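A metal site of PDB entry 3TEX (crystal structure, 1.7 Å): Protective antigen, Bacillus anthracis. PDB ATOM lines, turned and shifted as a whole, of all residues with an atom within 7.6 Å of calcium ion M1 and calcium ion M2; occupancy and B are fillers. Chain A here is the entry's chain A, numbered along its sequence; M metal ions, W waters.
N of Asp 179 lies close to O of Pro 223. OD2 of Asp 177 is in hydrogen-bond range of N of Gly 182 (2.9 Å). OD1 of Asp 185 sits close to N of Asp 177, at 3.3 Å. O of Glu 188 is in hydrogen-bond range of N of Ser 221, at 3.1 Å. The side-chain carboxylate (OD1) of Asp 235 sits at hydrogen-bond distance from the backbone NH (N) of Thr 228 (2.8 Å). OG of Ser 222 sits at hydrogen-bond distance from N of Lys 225 (3.2 Å). OG1 of Thr 228 sits at hydrogen-bond distance from N of Ser 222 (2.9 Å). N of Glu 224 lies within hydrogen-bond range of OG of Ser 222, 3.0 Å away.
Residues that only touch calcium ion M1: Thr 228 (3.95 Å). Seven residues have an atom within 4 Å of calcium ion M1: Asp 179, Asp 181, Glu 188, Ser 222, Lys 225, Thr 228 and Asp 235. The nearest printed residue that does not touch calcium ion M1 is Trp 226 (4.1 Å).
Within 4 Å of calcium ion M2: Asp 177, Asp 179, Asp 181, Ile 183 and Glu 188.
Calcium ion M1 is bound by OD2 of Asp 179 (2.3 Å), OD2 of Asp 235 (2.4 Å), OD2 of Asp 181 (2.4 Å), O of Ser 222 (2.4 Å), O of Lys 225 (2.4 Å), OE1 of Glu 188 (2.4 Å) and OE2 of Glu 188 (2.9 Å). Calcium ion M1 has seven donor atoms within binding distance.
Calcium ion M2 is bound by the backbone carbonyl oxygen of Ile 183 (2.3 Å), the side-chain carboxylate of Asp 177 (2.3 Å), the side-chain carboxylate of Glu 188 (2.3 Å), the side-chain carboxylate of Asp 179 (2.4 Å), the side-chain carboxylate of Asp 181 (2.4 Å) and water W1 (2.5 Å). Calcium ion M2 has six donor atoms within binding distance.
Water W1 lies within hydrogen-bond range of the backbone carbonyl oxygen (O) of Pro 223, the side-chain carboxylate (OD1) of Asp 185 and the backbone NH (N) of Arg 178.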
ATOM      1  N   TYR A  22      -3.787  22.227  42.557  1.00  0.00           N
ATOM      2  CA  TYR A  22      -3.894  21.063  41.697  1.00  0.00           C
ATOM      3  C   TYR A  22      -3.927  19.824  42.579  1.00  0.00           C
ATOM      4  O   TYR A  22      -2.990  19.570  43.330  1.00  0.00           O
ATOM      5  CB  TYR A  22      -2.693  20.987  40.767  1.00  0.00           C
ATOM      6  CG  TYR A  22      -2.565  22.176  39.863  1.00  0.00           C
ATOM      7  CD1 TYR A  22      -1.723  23.223  40.183  1.00  0.00           C
ATOM      8  CD2 TYR A  22      -3.310  22.270  38.698  1.00  0.00           C
ATOM      9  CE1 TYR A  22      -1.618  24.336  39.351  1.00  0.00           C
ATOM     10  CE2 TYR A  22      -3.215  23.361  37.870  1.00  0.00           C
ATOM     11  CZ  TYR A  22      -2.370  24.386  38.201  1.00  0.00           C
ATOM     12  OH  TYR A  22      -2.281  25.469  37.369  1.00  0.00           O
ATOM     13  N   PRO A 176       2.971  20.369  34.317  1.00  0.00           N
ATOM     14  CA  PRO A 176       3.111  20.804  32.927  1.00  0.00           C
ATOM     15  C   PRO A 176       1.990  21.774  32.550  1.00  0.00           C
ATOM     16  O   PRO A 176       0.823  21.406  32.599  1.00  0.00           O
ATOM     17  CB  PRO A 176       3.002  19.507  32.133  1.00  0.00           C
ATOM     18  CG  PRO A 176       3.359  18.413  33.125  1.00  0.00           C
ATOM     19  CD  PRO A 176       2.828  18.904  34.432  1.00  0.00           C
ATOM     20  N   ASP A 177       2.367  22.998  32.208  1.00  0.00           N
ATOM     21  CA  ASP A 177       1.438  24.045  31.820  1.00  0.00           C
ATOM     22  C   ASP A 177       2.234  24.938  30.874  1.00  0.00           C
ATOM     23  O   ASP A 177       2.622  26.053  31.243  1.00  0.00           O
ATOM     24  CB  ASP A 177       1.004  24.816  33.061  1.00  0.00           C
ATOM     25  CG  ASP A 177       0.014  25.911  32.748  1.00  0.00           C
ATOM     26  OD1 ASP A 177      -0.626  25.799  31.679  1.00  0.00           O
ATOM     27  OD2 ASP A 177      -0.148  26.849  33.548  1.00  0.00           O
ATOM     28  N   ARG A 178       2.511  24.417  29.685  1.00  0.00           N
ATOM     29  CA  ARG A 178       3.429  25.028  28.722  1.00  0.00           C
ATOM     30  C   ARG A 178       3.067  26.484  28.364  1.00  0.00           C
ATOM     31  O   ARG A 178       3.954  27.301  28.131  1.00  0.00           O
ATOM     32  CB  ARG A 178       3.502  24.144  27.449  1.00  0.00           C
ATOM     33  CG  ARG A 178       4.021  22.704  27.702  1.00  0.00           C
ATOM     34  CD  ARG A 178       3.679  21.720  26.575  1.00  0.00           C
ATOM     35  NE  ARG A 178       4.634  21.748  25.458  1.00  0.00           N
ATOM     36  CZ  ARG A 178       5.876  21.302  25.542  1.00  0.00           C
ATOM     37  NH1 ARG A 178       6.316  20.806  26.689  1.00  0.00           N
ATOM     38  NH2 ARG A 178       6.679  21.357  24.491  1.00  0.00           N
ATOM     39  N   ASP A 179       1.775  26.809  28.344  1.00  0.00           N
ATOM     40  CA  ASP A 179       1.344  28.163  27.970  1.00  0.00           C
ATOM     41  C   ASP A 179       1.028  29.087  29.167  1.00  0.00           C
ATOM     42  O   ASP A 179       0.614  30.229  29.001  1.00  0.00           O
ATOM     43  CB  ASP A 179       0.147  28.094  27.017  1.00  0.00           C
ATOM     44  CG  ASP A 179      -1.018  27.343  27.606  1.00  0.00           C
ATOM     45  OD1 ASP A 179      -1.010  27.078  28.831  1.00  0.00           O
ATOM     46  OD2 ASP A 179      -1.951  27.015  26.845  1.00  0.00           O
ATOM     47  N   ASN A 180       1.220  28.586  30.379  1.00  0.00           N
ATOM     48  CA  ASN A 180       0.966  29.364  31.573  1.00  0.00           C
ATOM     49  C   ASN A 180      -0.453  29.918  31.723  1.00  0.00           C
ATOM     50  O   ASN A 180      -0.650  30.981  32.320  1.00  0.00           O
ATOM     51  CB  ASN A 180       1.943  30.539  31.694  1.00  0.00           C
ATOM     52  CG  ASN A 180       2.162  30.968  33.145  1.00  0.00           C
ATOM     53  OD1 ASN A 180       2.270  30.128  34.033  1.00  0.00           O
ATOM     54  ND2 ASN A 180       2.200  32.269  33.379  1.00  0.00           N
ATOM     55  N   ASP A 181      -1.467  29.229  31.204  1.00  0.00           N
ATOM     56  CA  ASP A 181      -2.806  29.730  31.486  1.00  0.00           C
ATOM     57  C   ASP A 181      -3.359  29.197  32.792  1.00  0.00           C
ATOM     58  O   ASP A 181      -4.370  29.697  33.284  1.00  0.00           O
ATOM     59  CB  ASP A 181      -3.793  29.532  30.315  1.00  0.00           C
ATOM     60  CG  ASP A 181      -3.943  28.088  29.899  1.00  0.00           C
ATOM     61  OD1 ASP A 181      -3.669  27.144  30.686  1.00  0.00           O
ATOM     62  OD2 ASP A 181      -4.364  27.874  28.748  1.00  0.00           O
ATOM     63  N   GLY A 182      -2.694  28.199  33.369  1.00  0.00           N
ATOM     64  CA  GLY A 182      -3.197  27.555  34.576  1.00  0.00           C
ATOM     65  C   GLY A 182      -3.793  26.167  34.397  1.00  0.00           C
ATOM     66  O   GLY A 182      -3.840  25.398  35.354  1.00  0.00           O
ATOM     67  N   ILE A 183      -4.240  25.828  33.184  1.00  0.00           N
ATOM     68  CA  ILE A 183      -4.805  24.502  32.947  1.00  0.00           C
ATOM     69  C   ILE A 183      -3.692  23.549  32.524  1.00  0.00           C
ATOM     70  O   ILE A 183      -2.994  23.805  31.562  1.00  0.00           O
ATOM     71  CB  ILE A 183      -5.867  24.537  31.838  1.00  0.00           C
ATOM     72  CG1 ILE A 183      -6.894  25.648  32.106  1.00  0.00           C
ATOM     73  CG2 ILE A 183      -6.562  23.173  31.732  1.00  0.00           C
ATOM     74  CD1 ILE A 183      -7.902  25.866  30.966  1.00  0.00           C
ATOM     75  N   PRO A 184      -3.504  22.446  33.270  1.00  0.00           N
ATOM     76  CA  PRO A 184      -2.464  21.476  32.931  1.00  0.00           C
ATOM     77  C   PRO A 184      -2.563  20.990  31.486  1.00  0.00           C
ATOM     78  O   PRO A 184      -3.679  20.790  30.981  1.00  0.00           O
ATOM     79  CB  PRO A 184      -2.751  20.322  33.898  1.00  0.00           C
ATOM     80  CG  PRO A 184      -3.322  21.008  35.110  1.00  0.00           C
ATOM     81  CD  PRO A 184      -4.186  22.121  34.535  1.00  0.00           C
ATOM     82  N   ASP A 185      -1.416  20.808  30.826  1.00  0.00           N
ATOM     83  CA  ASP A 185      -1.353  20.277  29.457  1.00  0.00           C
ATOM     84  C   ASP A 185      -2.355  19.143  29.222  1.00  0.00           C
ATOM     85  O   ASP A 185      -3.139  19.164  28.270  1.00  0.00           O
ATOM     86  CB  ASP A 185       0.027  19.680  29.164  1.00  0.00           C
ATOM     87  CG  ASP A 185       1.145  20.710  29.143  1.00  0.00           C
ATOM     88  OD1 ASP A 185       0.920  21.906  29.414  1.00  0.00           O
ATOM     89  OD2 ASP A 185       2.300  20.289  28.879  1.00  0.00           O
ATOM     90  N   SER A 186      -2.285  18.119  30.070  1.00  0.00           N
ATOM     91  CA  SER A 186      -3.042  16.907  29.851  1.00  0.00           C
ATOM     92  C   SER A 186      -4.549  17.141  29.826  1.00  0.00           C
ATOM     93  O   SER A 186      -5.260  16.479  29.077  1.00  0.00           O
ATOM     94  CB  SER A 186      -2.681  15.845  30.906  1.00  0.00           C
ATOM     95  OG  SER A 186      -2.904  16.327  32.215  1.00  0.00           O
ATOM     96  N   GLU A 188      -6.105  20.027  28.946  1.00  0.00           N
ATOM     97  CA  GLU A 188      -6.459  20.781  27.735  1.00  0.00           C
ATOM     98  C   GLU A 188      -6.539  19.854  26.533  1.00  0.00           C
ATOM     99  O   GLU A 188      -7.426  19.996  25.685  1.00  0.00           O
ATOM    100  CB  GLU A 188      -5.433  21.892  27.474  1.00  0.00           C
ATOM    101  CG  GLU A 188      -5.431  22.980  28.521  1.00  0.00           C
ATOM    102  CD  GLU A 188      -4.881  24.285  27.985  1.00  0.00           C
ATOM    103  OE1 GLU A 188      -5.578  24.928  27.168  1.00  0.00           O
ATOM    104  OE2 GLU A 188      -3.753  24.664  28.376  1.00  0.00           O
ATOM    105  N   TYR A 192     -11.838  18.568  29.463  1.00  0.00           N
ATOM    106  CA  TYR A 192     -12.125  18.920  30.848  1.00  0.00           C
ATOM    107  C   TYR A 192     -13.501  19.544  30.961  1.00  0.00           C
ATOM    108  O   TYR A 192     -14.101  19.969  29.970  1.00  0.00           O
ATOM    109  CB  TYR A 192     -11.083  19.894  31.390  1.00  0.00           C
ATOM    110  CG  TYR A 192     -10.847  21.149  30.567  1.00  0.00           C
ATOM    111  CD1 TYR A 192     -10.065  21.111  29.414  1.00  0.00           C
ATOM    112  CD2 TYR A 192     -11.339  22.375  30.989  1.00  0.00           C
ATOM    113  CE1 TYR A 192      -9.827  22.275  28.674  1.00  0.00           C
ATOM    114  CE2 TYR A 192     -11.106  23.553  30.259  1.00  0.00           C
ATOM    115  CZ  TYR A 192     -10.328  23.486  29.113  1.00  0.00           C
ATOM    116  OH  TYR A 192     -10.087  24.628  28.385  1.00  0.00           O
ATOM    117  N   SER A 221      -8.769  22.512  24.588  1.00  0.00           N
ATOM    118  CA  SER A 221      -8.061  23.713  24.166  1.00  0.00           C
ATOM    119  C   SER A 221      -6.601  23.398  23.878  1.00  0.00           C
ATOM    120  O   SER A 221      -6.144  22.307  24.166  1.00  0.00           O
ATOM    121  CB  SER A 221      -8.179  24.814  25.238  1.00  0.00           C
ATOM    122  OG  SER A 221      -8.063  24.273  26.555  1.00  0.00           O
ATOM    123  N   SER A 222      -5.868  24.328  23.281  1.00  0.00           N
ATOM    124  CA  SER A 222      -4.444  24.065  23.025  1.00  0.00           C
ATOM    125  C   SER A 222      -3.605  24.262  24.285  1.00  0.00           C
ATOM    126  O   SER A 222      -3.658  25.297  24.903  1.00  0.00           O
ATOM    127  CB  SER A 222      -3.884  24.981  21.947  1.00  0.00           C
ATOM    128  OG  SER A 222      -2.467  24.822  21.940  1.00  0.00           O
ATOM    129  N   PRO A 223      -2.778  23.269  24.620  1.00  0.00           N
ATOM    130  CA  PRO A 223      -1.874  23.392  25.770  1.00  0.00           C
ATOM    131  C   PRO A 223      -0.717  24.363  25.499  1.00  0.00           C
ATOM    132  O   PRO A 223       0.073  24.687  26.397  1.00  0.00           O
ATOM    133  CB  PRO A 223      -1.352  21.965  25.945  1.00  0.00           C
ATOM    134  CG  PRO A 223      -1.358  21.403  24.556  1.00  0.00           C
ATOM    135  CD  PRO A 223      -2.631  21.975  23.936  1.00  0.00           C
ATOM    136  N   GLU A 224      -0.625  24.848  24.261  1.00  0.00           N
ATOM    137  CA  GLU A 224       0.458  25.743  23.882  1.00  0.00           C
ATOM    138  C   GLU A 224      -0.004  27.154  23.474  1.00  0.00           C
ATOM    139  O   GLU A 224       0.805  28.029  23.146  1.00  0.00           O
ATOM    140  CB  GLU A 224       1.295  25.073  22.789  1.00  0.00           C
ATOM    141  CG  GLU A 224       1.929  23.785  23.330  1.00  0.00           C
ATOM    142  CD  GLU A 224       2.844  23.083  22.359  1.00  0.00           C
ATOM    143  OE1 GLU A 224       3.245  23.721  21.358  1.00  0.00           O
ATOM    144  OE2 GLU A 224       3.182  21.902  22.604  1.00  0.00           O
ATOM    145  N   LYS A 225      -1.316  27.380  23.536  1.00  0.00           N
ATOM    146  CA  LYS A 225      -1.855  28.701  23.352  1.00  0.00           C
ATOM    147  C   LYS A 225      -2.564  29.176  24.615  1.00  0.00           C
ATOM    148  O   LYS A 225      -3.524  28.561  25.068  1.00  0.00           O
ATOM    149  CB  LYS A 225      -2.829  28.717  22.176  1.00  0.00           C
ATOM    150  CG  LYS A 225      -2.179  28.334  20.856  1.00  0.00           C
ATOM    151  CD  LYS A 225      -3.231  28.300  19.734  1.00  0.00           C
ATOM    152  CE  LYS A 225      -3.800  29.687  19.471  1.00  0.00           C
ATOM    153  NZ  LYS A 225      -2.848  30.568  18.750  1.00  0.00           N
ATOM    154  N   TRP A 226      -2.074  30.270  25.178  1.00  0.00           N
ATOM    155  CA  TRP A 226      -2.639  30.858  26.383  1.00  0.00           C
ATOM    156  C   TRP A 226      -4.115  31.200  26.144  1.00  0.00           C
ATOM    157  O   TRP A 226      -4.976  30.921  26.978  1.00  0.00           O
ATOM    158  CB  TRP A 226      -1.813  32.094  26.736  1.00  0.00           C
ATOM    159  CG  TRP A 226      -2.236  32.883  27.927  1.00  0.00           C
ATOM    160  CD1 TRP A 226      -1.885  32.649  29.235  1.00  0.00           C
ATOM    161  CD2 TRP A 226      -3.049  34.053  27.930  1.00  0.00           C
ATOM    162  NE1 TRP A 226      -2.454  33.596  30.047  1.00  0.00           N
ATOM    163  CE2 TRP A 226      -3.159  34.483  29.274  1.00  0.00           C
ATOM    164  CE3 TRP A 226      -3.696  34.789  26.921  1.00  0.00           C
ATOM    165  CZ2 TRP A 226      -3.906  35.612  29.634  1.00  0.00           C
ATOM    166  CZ3 TRP A 226      -4.431  35.919  27.288  1.00  0.00           C
ATOM    167  CH2 TRP A 226      -4.527  36.321  28.637  1.00  0.00           C
ATOM    168  N   SER A 227      -4.396  31.820  24.997  1.00  0.00           N
ATOM    169  CA  SER A 227      -5.759  31.917  24.485  1.00  0.00           C
ATOM    170  C   SER A 227      -5.838  31.116  23.204  1.00  0.00           C
ATOM    171  O   SER A 227      -5.178  31.451  22.204  1.00  0.00           O
ATOM    172  CB  SER A 227      -6.149  33.360  24.191  1.00  0.00           C
ATOM    173  OG  SER A 227      -7.446  33.423  23.621  1.00  0.00           O
ATOM    174  N   THR A 228      -6.631  30.058  23.211  1.00  0.00           N
ATOM    175  CA  THR A 228      -6.678  29.158  22.065  1.00  0.00           C
ATOM    176  C   THR A 228      -7.318  29.837  20.846  1.00  0.00           C
ATOM    177  O   THR A 228      -6.963  29.536  19.724  1.00  0.00           O
ATOM    178  CB  THR A 228      -7.359  27.827  22.431  1.00  0.00           C
ATOM    179  OG1 THR A 228      -6.485  27.119  23.341  1.00  0.00           O
ATOM    180  CG2 THR A 228      -7.562  26.958  21.199  1.00  0.00           C
ATOM    181  N   SER A 234      -7.549  34.412  28.548  1.00  0.00           N
ATOM    182  CA  SER A 234      -6.965  33.083  28.583  1.00  0.00           C
ATOM    183  C   SER A 234      -7.999  31.953  28.689  1.00  0.00           C
ATOM    184  O   SER A 234      -9.137  32.173  29.115  1.00  0.00           O
ATOM    185  CB  SER A 234      -5.957  32.936  29.719  1.00  0.00           C
ATOM    186  OG  SER A 234      -6.540  32.328  30.851  1.00  0.00           O
ATOM    187  N   ASP A 235      -7.573  30.747  28.324  1.00  0.00           N
ATOM    188  CA  ASP A 235      -8.481  29.596  28.337  1.00  0.00           C
ATOM    189  C   ASP A 235      -9.040  29.382  29.753  1.00  0.00           C
ATOM    190  O   ASP A 235     -10.216  29.103  29.956  1.00  0.00           O
ATOM    191  CB  ASP A 235      -7.740  28.355  27.835  1.00  0.00           C
ATOM    192  CG  ASP A 235      -7.310  28.457  26.381  1.00  0.00           C
ATOM    193  OD1 ASP A 235      -7.926  29.222  25.600  1.00  0.00           O
ATOM    194  OD2 ASP A 235      -6.376  27.716  26.005  1.00  0.00           O
ATOM    195  N   PHE A 236      -8.175  29.584  30.739  1.00  0.00           N
ATOM    196  CA  PHE A 236      -8.539  29.462  32.136  1.00  0.00           C
ATOM    197  C   PHE A 236      -9.425  30.602  32.626  1.00  0.00           C
ATOM    198  O   PHE A 236     -10.396  30.365  33.366  1.00  0.00           O
ATOM    199  CB  PHE A 236      -7.240  29.397  32.961  1.00  0.00           C
ATOM    200  CG  PHE A 236      -7.448  29.243  34.444  1.00  0.00           C
ATOM    201  CD1 PHE A 236      -7.794  28.021  34.989  1.00  0.00           C
ATOM    202  CD2 PHE A 236      -7.190  30.303  35.299  1.00  0.00           C
ATOM    203  CE1 PHE A 236      -7.942  27.864  36.367  1.00  0.00           C
ATOM    204  CE2 PHE A 236      -7.338  30.167  36.691  1.00  0.00           C
ATOM    205  CZ  PHE A 236      -7.708  28.930  37.221  1.00  0.00           C
ATOM    206  N   PRO A 254     -13.284  28.288  25.310  1.00  0.00           N
ATOM    207  CA  PRO A 254     -11.934  28.563  24.789  1.00  0.00           C
ATOM    208  C   PRO A 254     -11.805  28.465  23.270  1.00  0.00           C
ATOM    209  O   PRO A 254     -10.816  28.988  22.742  1.00  0.00           O
ATOM    210  CB  PRO A 254     -11.067  27.492  25.485  1.00  0.00           C
ATOM    211  CG  PRO A 254     -11.764  27.250  26.773  1.00  0.00           C
ATOM    212  CD  PRO A 254     -13.249  27.301  26.419  1.00  0.00           C
HETATM  213 CA    CA M   1      -4.256  26.866  26.593  1.00  0.00          CA
HETATM  214 CA    CA M   2      -2.185  25.323  29.994  1.00  0.00          CA
HETATM  215  O   HOH W   1      -0.675  23.834  28.714  1.00  0.00           O
